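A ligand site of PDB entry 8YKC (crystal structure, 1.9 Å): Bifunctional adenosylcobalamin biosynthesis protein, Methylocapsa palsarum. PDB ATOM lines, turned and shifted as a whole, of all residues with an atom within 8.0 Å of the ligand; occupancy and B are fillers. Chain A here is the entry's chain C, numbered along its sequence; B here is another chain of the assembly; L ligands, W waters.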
ATOM      1  N   VAL A  16      10.411  10.529  -8.590  1.00  0.00           N
ATOM      2  CA  VAL A  16      11.657   9.736  -8.808  1.00  0.00           C
ATOM      3  C   VAL A  16      12.747  10.361  -7.947  1.00  0.00           C
ATOM      4  O   VAL A  16      13.040  11.559  -8.128  1.00  0.00           O
ATOM      5  CB  VAL A  16      12.096   9.695 -10.280  1.00  0.00           C
ATOM      6  CG1 VAL A  16      13.332   8.830 -10.450  1.00  0.00           C
ATOM      7  CG2 VAL A  16      10.974   9.197 -11.181  1.00  0.00           C
ATOM      8  N   VAL A  17      13.278   9.604  -7.004  1.00  0.00           N
ATOM      9  CA  VAL A  17      14.314  10.138  -6.085  1.00  0.00           C
ATOM     10  C   VAL A  17      15.600   9.342  -6.280  1.00  0.00           C
ATOM     11  O   VAL A  17      15.594   8.082  -6.176  1.00  0.00           O
ATOM     12  CB  VAL A  17      13.816  10.109  -4.633  1.00  0.00           C
ATOM     13  CG1 VAL A  17      14.907  10.538  -3.685  1.00  0.00           C
ATOM     14  CG2 VAL A  17      12.558  10.957  -4.471  1.00  0.00           C
ATOM     15  N   GLY A  18      16.706  10.073  -6.427  1.00  0.00           N
ATOM     16  CA  GLY A  18      18.043   9.473  -6.309  1.00  0.00           C
ATOM     17  C   GLY A  18      19.109  10.497  -5.996  1.00  0.00           C
ATOM     18  O   GLY A  18      18.816  11.719  -5.986  1.00  0.00           O
ATOM     19  N   GLY A  19      20.326   9.986  -5.788  1.00  0.00           N
ATOM     20  CA  GLY A  19      21.525  10.793  -5.547  1.00  0.00           C
ATOM     21  C   GLY A  19      22.024  11.423  -6.848  1.00  0.00           C
ATOM     22  O   GLY A  19      21.335  11.329  -7.908  1.00  0.00           O
ATOM     23  N   ALA A  20      23.132  12.143  -6.743  1.00  0.00           N
ATOM     24  CA  ALA A  20      23.782  12.794  -7.896  1.00  0.00           C
ATOM     25  C   ALA A  20      24.266  11.708  -8.858  1.00  0.00           C
ATOM     26  O   ALA A  20      24.876  10.718  -8.404  1.00  0.00           O
ATOM     27  CB  ALA A  20      24.907  13.684  -7.426  1.00  0.00           C
ATOM     28  N   ARG A  21      23.984  11.887 -10.150  1.00  0.00           N
ATOM     29  CA  ARG A  21      24.334  10.910 -11.209  1.00  0.00           C
ATOM     30  C   ARG A  21      23.915   9.498 -10.764  1.00  0.00           C
ATOM     31  O   ARG A  21      24.724   8.567 -10.755  1.00  0.00           O
ATOM     32  CB  ARG A  21      25.815  11.049 -11.573  1.00  0.00           C
ATOM     33  CG  ARG A  21      26.063  12.171 -12.579  1.00  0.00           C
ATOM     34  CD  ARG A  21      25.768  11.731 -13.997  1.00  0.00           C
ATOM     35  NE  ARG A  21      26.275  12.682 -14.984  1.00  0.00           N
ATOM     36  CZ  ARG A  21      27.509  12.690 -15.512  1.00  0.00           C
ATOM     37  NH1 ARG A  21      28.406  11.790 -15.164  1.00  0.00           N
ATOM     38  NH2 ARG A  21      27.819  13.625 -16.391  1.00  0.00           N
ATOM     39  N   SER A  22      22.639   9.376 -10.432  1.00  0.00           N
ATOM     40  CA  SER A  22      22.008   8.106 -10.003  1.00  0.00           C
ATOM     41  C   SER A  22      21.418   7.392 -11.224  1.00  0.00           C
ATOM     42  O   SER A  22      21.119   6.211 -11.112  1.00  0.00           O
ATOM     43  CB  SER A  22      20.984   8.381  -8.935  1.00  0.00           C
ATOM     44  OG  SER A  22      20.005   9.337  -9.344  1.00  0.00           O
ATOM     45  N   GLY A  23      21.244   8.076 -12.351  1.00  0.00           N
ATOM     46  CA  GLY A  23      20.456   7.548 -13.485  1.00  0.00           C
ATOM     47  C   GLY A  23      18.969   7.905 -13.395  1.00  0.00           C
ATOM     48  O   GLY A  23      18.211   7.418 -14.255  1.00  0.00           O
ATOM     49  N   LYS A  24      18.553   8.752 -12.454  1.00  0.00           N
ATOM     50  CA  LYS A  24      17.101   9.086 -12.263  1.00  0.00           C
ATOM     51  C   LYS A  24      16.557   9.932 -13.430  1.00  0.00           C
ATOM     52  O   LYS A  24      15.398   9.676 -13.826  1.00  0.00           O
ATOM     53  CB  LYS A  24      16.886   9.838 -10.947  1.00  0.00           C
ATOM     54  CG  LYS A  24      17.568  11.192 -10.827  1.00  0.00           C
ATOM     55  CD  LYS A  24      17.487  11.755  -9.432  1.00  0.00           C
ATOM     56  CE  LYS A  24      18.101  13.128  -9.310  1.00  0.00           C
ATOM     57  NZ  LYS A  24      19.510  13.098  -9.743  1.00  0.00           N
ATOM     58  N   SER A  25      17.293  10.937 -13.909  1.00  0.00           N
ATOM     59  CA  SER A  25      16.902  11.800 -15.059  1.00  0.00           C
ATOM     60  C   SER A  25      16.565  10.945 -16.283  1.00  0.00           C
ATOM     61  O   SER A  25      15.447  11.102 -16.841  1.00  0.00           O
ATOM     62  CB  SER A  25      17.969  12.807 -15.405  1.00  0.00           C
ATOM     63  OG  SER A  25      17.931  13.895 -14.517  1.00  0.00           O
ATOM     64  N   ARG A  26      17.466  10.038 -16.676  1.00  0.00           N
ATOM     65  CA  ARG A  26      17.255   9.151 -17.860  1.00  0.00           C
ATOM     66  C   ARG A  26      16.165   8.122 -17.534  1.00  0.00           C
ATOM     67  O   ARG A  26      15.483   7.657 -18.476  1.00  0.00           O
ATOM     68  CB  ARG A  26      18.576   8.494 -18.289  1.00  0.00           C
ATOM     69  CG  ARG A  26      18.732   8.308 -19.793  1.00  0.00           C
ATOM     70  CD  ARG A  26      19.582   7.108 -20.193  1.00  0.00           C
ATOM     71  NE  ARG A  26      18.943   5.840 -19.849  1.00  0.00           N
ATOM     72  CZ  ARG A  26      19.199   5.085 -18.765  1.00  0.00           C
ATOM     73  NH1 ARG A  26      20.103   5.464 -17.871  1.00  0.00           N
ATOM     74  NH2 ARG A  26      18.542   3.954 -18.574  1.00  0.00           N
ATOM     75  N   PHE A  27      15.974   7.735 -16.270  1.00  0.00           N
ATOM     76  CA  PHE A  27      14.860   6.831 -15.898  1.00  0.00           C
ATOM     77  C   PHE A  27      13.519   7.531 -16.162  1.00  0.00           C
ATOM     78  O   PHE A  27      12.615   6.897 -16.755  1.00  0.00           O
ATOM     79  CB  PHE A  27      14.948   6.375 -14.436  1.00  0.00           C
ATOM     80  CG  PHE A  27      13.771   5.526 -14.016  1.00  0.00           C
ATOM     81  CD1 PHE A  27      13.628   4.226 -14.462  1.00  0.00           C
ATOM     82  CD2 PHE A  27      12.796   6.043 -13.176  1.00  0.00           C
ATOM     83  CE1 PHE A  27      12.533   3.452 -14.094  1.00  0.00           C
ATOM     84  CE2 PHE A  27      11.709   5.258 -12.812  1.00  0.00           C
ATOM     85  CZ  PHE A  27      11.577   3.966 -13.253  1.00  0.00           C
ATOM     86  N   ALA A  28      13.373   8.785 -15.722  1.00  0.00           N
ATOM     87  CA  ALA A  28      12.135   9.592 -15.852  1.00  0.00           C
ATOM     88  C   ALA A  28      11.848   9.848 -17.340  1.00  0.00           C
ATOM     89  O   ALA A  28      10.706   9.562 -17.777  1.00  0.00           O
ATOM     90  CB  ALA A  28      12.249  10.876 -15.104  1.00  0.00           C
ATOM     91  N   ASP A  93      12.301  18.727 -14.311  1.00  0.00           N
ATOM     92  CA  ASP A  93      13.709  18.355 -14.583  1.00  0.00           C
ATOM     93  C   ASP A  93      14.451  18.219 -13.253  1.00  0.00           C
ATOM     94  O   ASP A  93      15.121  17.190 -13.055  1.00  0.00           O
ATOM     95  CB  ASP A  93      14.404  19.360 -15.494  1.00  0.00           C
ATOM     96  CG  ASP A  93      15.850  18.989 -15.645  1.00  0.00           C
ATOM     97  OD1 ASP A  93      16.541  19.024 -14.628  1.00  0.00           O
ATOM     98  OD2 ASP A  93      16.251  18.590 -16.762  1.00  0.00           O
ATOM     99  N   SER A  94      14.354  19.240 -12.394  1.00  0.00           N
ATOM    100  CA  SER A  94      14.721  19.190 -10.962  1.00  0.00           C
ATOM    101  C   SER A  94      13.725  19.985 -10.136  1.00  0.00           C
ATOM    102  O   SER A  94      13.619  21.224 -10.288  1.00  0.00           O
ATOM    103  CB  SER A  94      16.109  19.697 -10.680  1.00  0.00           C
ATOM    104  OG  SER A  94      17.042  18.632 -10.702  1.00  0.00           O
ATOM    105  N   LEU A  97      16.348  22.363  -8.043  1.00  0.00           N
ATOM    106  CA  LEU A  97      16.847  23.708  -8.454  1.00  0.00           C
ATOM    107  C   LEU A  97      15.780  24.773  -8.217  1.00  0.00           C
ATOM    108  O   LEU A  97      16.155  25.923  -7.854  1.00  0.00           O
ATOM    109  CB  LEU A  97      17.256  23.601  -9.910  1.00  0.00           C
ATOM    110  CG  LEU A  97      18.142  22.384 -10.196  1.00  0.00           C
ATOM    111  CD1 LEU A  97      18.139  22.073 -11.684  1.00  0.00           C
ATOM    112  CD2 LEU A  97      19.565  22.596  -9.691  1.00  0.00           C
ATOM    113  N   VAL A 130      11.245  14.861 -10.841  1.00  0.00           N
ATOM    114  CA  VAL A 130      12.602  14.267 -10.633  1.00  0.00           C
ATOM    115  C   VAL A 130      13.279  15.080  -9.528  1.00  0.00           C
ATOM    116  O   VAL A 130      13.242  16.325  -9.609  1.00  0.00           O
ATOM    117  CB  VAL A 130      13.448  14.209 -11.921  1.00  0.00           C
ATOM    118  CG1 VAL A 130      14.751  13.449 -11.683  1.00  0.00           C
ATOM    119  CG2 VAL A 130      12.666  13.576 -13.062  1.00  0.00           C
ATOM    120  N   SER A 131      13.769  14.407  -8.482  1.00  0.00           N
ATOM    121  CA  SER A 131      14.292  15.076  -7.261  1.00  0.00           C
ATOM    122  C   SER A 131      15.504  14.290  -6.729  1.00  0.00           C
ATOM    123  O   SER A 131      15.588  13.056  -6.919  1.00  0.00           O
ATOM    124  CB  SER A 131      13.174  15.250  -6.238  1.00  0.00           C
ATOM    125  OG  SER A 131      13.429  16.278  -5.265  1.00  0.00           O
ATOM    126  N   ASN A 132      16.386  14.985  -6.060  1.00  0.00           N
ATOM    127  CA  ASN A 132      17.598  14.433  -5.408  1.00  0.00           C
ATOM    128  C   ASN A 132      17.306  14.080  -3.945  1.00  0.00           C
ATOM    129  O   ASN A 132      16.623  14.852  -3.277  1.00  0.00           O
ATOM    130  CB  ASN A 132      18.758  15.430  -5.452  1.00  0.00           C
ATOM    131  CG  ASN A 132      19.500  15.411  -6.775  1.00  0.00           C
ATOM    132  OD1 ASN A 132      20.636  14.925  -6.886  1.00  0.00           O
ATOM    133  ND2 ASN A 132      18.858  15.947  -7.777  1.00  0.00           N
ATOM    134  N   VAL A 169      15.848   5.539  -7.370  1.00  0.00           N
ATOM    135  CA  VAL A 169      16.863   5.136  -8.379  1.00  0.00           C
ATOM    136  C   VAL A 169      18.255   5.147  -7.738  1.00  0.00           C
ATOM    137  O   VAL A 169      18.710   6.231  -7.287  1.00  0.00           O
ATOM    138  CB  VAL A 169      16.782   6.036  -9.621  1.00  0.00           C
ATOM    139  CG1 VAL A 169      17.735   5.550 -10.676  1.00  0.00           C
ATOM    140  CG2 VAL A 169      15.368   6.102 -10.149  1.00  0.00           C
ATOM    141  N   GLY A 172      21.435   3.614 -11.262  1.00  0.00           N
ATOM    142  CA  GLY A 172      20.707   3.419 -12.524  1.00  0.00           C
ATOM    143  C   GLY A 172      19.592   2.399 -12.411  1.00  0.00           C
ATOM    144  O   GLY A 172      18.975   2.099 -13.436  1.00  0.00           O
ATOM    145  N   GLY B 135      26.643   9.969  -3.652  1.00  0.00           N
ATOM    146  CA  GLY B 135      25.783  10.944  -4.344  1.00  0.00           C
ATOM    147  C   GLY B 135      24.632  11.499  -3.513  1.00  0.00           C
ATOM    148  O   GLY B 135      23.974  12.350  -4.012  1.00  0.00           O
ATOM    149  N   ARG B 149      32.421  12.914  -7.273  1.00  0.00           N
ATOM    150  CA  ARG B 149      30.993  12.569  -6.982  1.00  0.00           C
ATOM    151  C   ARG B 149      30.276  12.160  -8.281  1.00  0.00           C
ATOM    152  O   ARG B 149      29.653  11.095  -8.330  1.00  0.00           O
ATOM    153  CB  ARG B 149      30.321  13.776  -6.353  1.00  0.00           C
ATOM    154  CG  ARG B 149      28.857  13.614  -5.964  1.00  0.00           C
ATOM    155  CD  ARG B 149      28.575  14.772  -5.035  1.00  0.00           C
ATOM    156  NE  ARG B 149      27.225  14.941  -4.535  1.00  0.00           N
ATOM    157  CZ  ARG B 149      26.280  15.684  -5.074  1.00  0.00           C
ATOM    158  NH1 ARG B 149      26.477  16.346  -6.213  1.00  0.00           N
ATOM    159  NH2 ARG B 149      25.106  15.757  -4.468  1.00  0.00           N
ATOM    160  N   ASP B 150      30.393  12.989  -9.321  1.00  0.00           N
ATOM    161  CA  ASP B 150      29.822  12.753 -10.672  1.00  0.00           C
ATOM    162  C   ASP B 150      30.315  11.423 -11.254  1.00  0.00           C
ATOM    163  O   ASP B 150      29.482  10.606 -11.707  1.00  0.00           O
ATOM    164  CB  ASP B 150      30.204  13.907 -11.581  1.00  0.00           C
ATOM    165  CG  ASP B 150      29.651  13.716 -12.967  1.00  0.00           C
ATOM    166  OD1 ASP B 150      28.458  14.043 -13.156  1.00  0.00           O
ATOM    167  OD2 ASP B 150      30.405  13.205 -13.833  1.00  0.00           O
ATOM    168  N   GLY B 153      29.217   8.178  -9.438  1.00  0.00           N
ATOM    169  CA  GLY B 153      27.811   7.890  -9.777  1.00  0.00           C
ATOM    170  C   GLY B 153      27.711   7.262 -11.167  1.00  0.00           C
ATOM    171  O   GLY B 153      27.108   6.182 -11.296  1.00  0.00           O
ATOM    172  N   MET B 154      28.361   7.870 -12.154  1.00  0.00           N
ATOM    173  CA  MET B 154      28.453   7.311 -13.535  1.00  0.00           C
ATOM    174  C   MET B 154      29.032   5.904 -13.444  1.00  0.00           C
ATOM    175  O   MET B 154      28.429   4.980 -14.007  1.00  0.00           O
ATOM    176  CB  MET B 154      29.314   8.212 -14.430  1.00  0.00           C
ATOM    177  CG  MET B 154      29.141   7.979 -15.922  1.00  0.00           C
ATOM    178  SD  MET B 154      30.340   6.780 -16.585  1.00  0.00           S
ATOM    179  CE  MET B 154      31.622   7.833 -17.262  1.00  0.00           C
ATOM    180  N   GLN B 157      26.566   3.277 -12.117  1.00  0.00           N
ATOM    181  CA  GLN B 157      25.516   3.050 -13.157  1.00  0.00           C
ATOM    182  C   GLN B 157      26.045   2.057 -14.209  1.00  0.00           C
ATOM    183  O   GLN B 157      25.338   1.081 -14.489  1.00  0.00           O
ATOM    184  CB  GLN B 157      25.114   4.335 -13.860  1.00  0.00           C
ATOM    185  CG  GLN B 157      24.333   5.301 -13.018  1.00  0.00           C
ATOM    186  CD  GLN B 157      23.962   6.490 -13.873  1.00  0.00           C
ATOM    187  OE1 GLN B 157      23.283   6.328 -14.872  1.00  0.00           O
ATOM    188  NE2 GLN B 157      24.442   7.666 -13.503  1.00  0.00           N
HETATM  189  P1  LIG L   1      22.442  14.465 -12.891  1.00  0.00           P
HETATM  190  O1  LIG L   1      22.455  14.710 -11.374  1.00  0.00           O
HETATM  191  O2  LIG L   1      23.814  14.572 -13.554  1.00  0.00           O
HETATM  192  O3  LIG L   1      21.398  15.272 -13.617  1.00  0.00           O
HETATM  193  O4  LIG L   1      22.139  12.911 -13.155  1.00  0.00           O
HETATM  194  P2  LIG L   1      21.101  11.760 -12.754  1.00  0.00           P
HETATM  195  O5  LIG L   1      21.588  10.581 -13.504  1.00  0.00           O
HETATM  196  O6  LIG L   1      19.744  12.247 -13.216  1.00  0.00           O
HETATM  197  O7  LIG L   1      21.204  11.635 -11.262  1.00  0.00           O
HETATM  198  O   HOH W   1      20.313  10.254 -15.637  1.00  0.00           O
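Water W1 bridges an oxygen (O5) of the ligand (2.5 Å) and the backbone NH (N) of Arg 26 (3.0 Å).
The side-chain hydroxyl (OG) of Ser 22 lies close to the backbone NH (N) of Lys 24 (3.5 Å).
The backbone carbonyl oxygen (O) of Gly 19 is in hydrogen-bond range of the side-chain amino group (NZ) of Lys 24.
The side-chain amide nitrogen (NE2) of Gln 157 of chain B lies close to the backbone NH (N) of Gly 23 (3.4 Å).
O of Gly 19 sits at hydrogen-bond distance from OG of Ser 22.
The backbone NH (N) of Gly 172 sits at hydrogen-bond distance from the backbone carbonyl oxygen (O) of Ser 22.
The backbone carbonyl oxygen of Arg 21 sits at hydrogen-bond distance from the side-chain amide nitrogen of Gln 157 of chain B (2.9 Å).
The guanidinium group (NH1) of Arg 21 is in salt-bridge range of the side-chain carboxylate (OD2) of Asp 150 of chain B (2.8 Å).
N of Ala 20 lies within hydrogen-bond range of O of Gly 135 of chain B (2.9 Å).
O7 of the ligand sits close to O of Gly 19, 3.4 Å away.
Merely in contact with the ligand: Ala 20.
Seven residues have an atom within 4 Å of the ligand: Gly 19, Ala 20, Arg 21, Ser 22, Gly 23, Lys 24 and Ser 25.
The nearest printed residue that does not touch the ligand is Gln 157 of chain B (4.1 Å).
The side-chain amino group of Lys 24 lies within salt-bridge range of an oxygen (O7) of the ligand, at 2.7 Å.
N of Ser 25 sits at hydrogen-bond distance from O6 of the ligand (2.9 Å).
OG of Ser 25 sits at hydrogen-bond distance from O6 of the ligand, at 2.8 Å.
N of Gly 23 lies within hydrogen-bond range of O5 of the ligand (2.8 Å).
The backbone NH (N) of Ser 22 is in hydrogen-bond range of an oxygen (O7) of the ligand (2.8 Å).
The side-chain hydroxyl (OG) of Ser 22 is in hydrogen-bond range of an oxygen (O7) of the ligand (3.2 Å).
O7 of the ligand lies within hydrogen-bond range of N of Arg 21 (3.0 Å).
NE of Arg 21 lies within salt-bridge range of O2 of the ligand.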
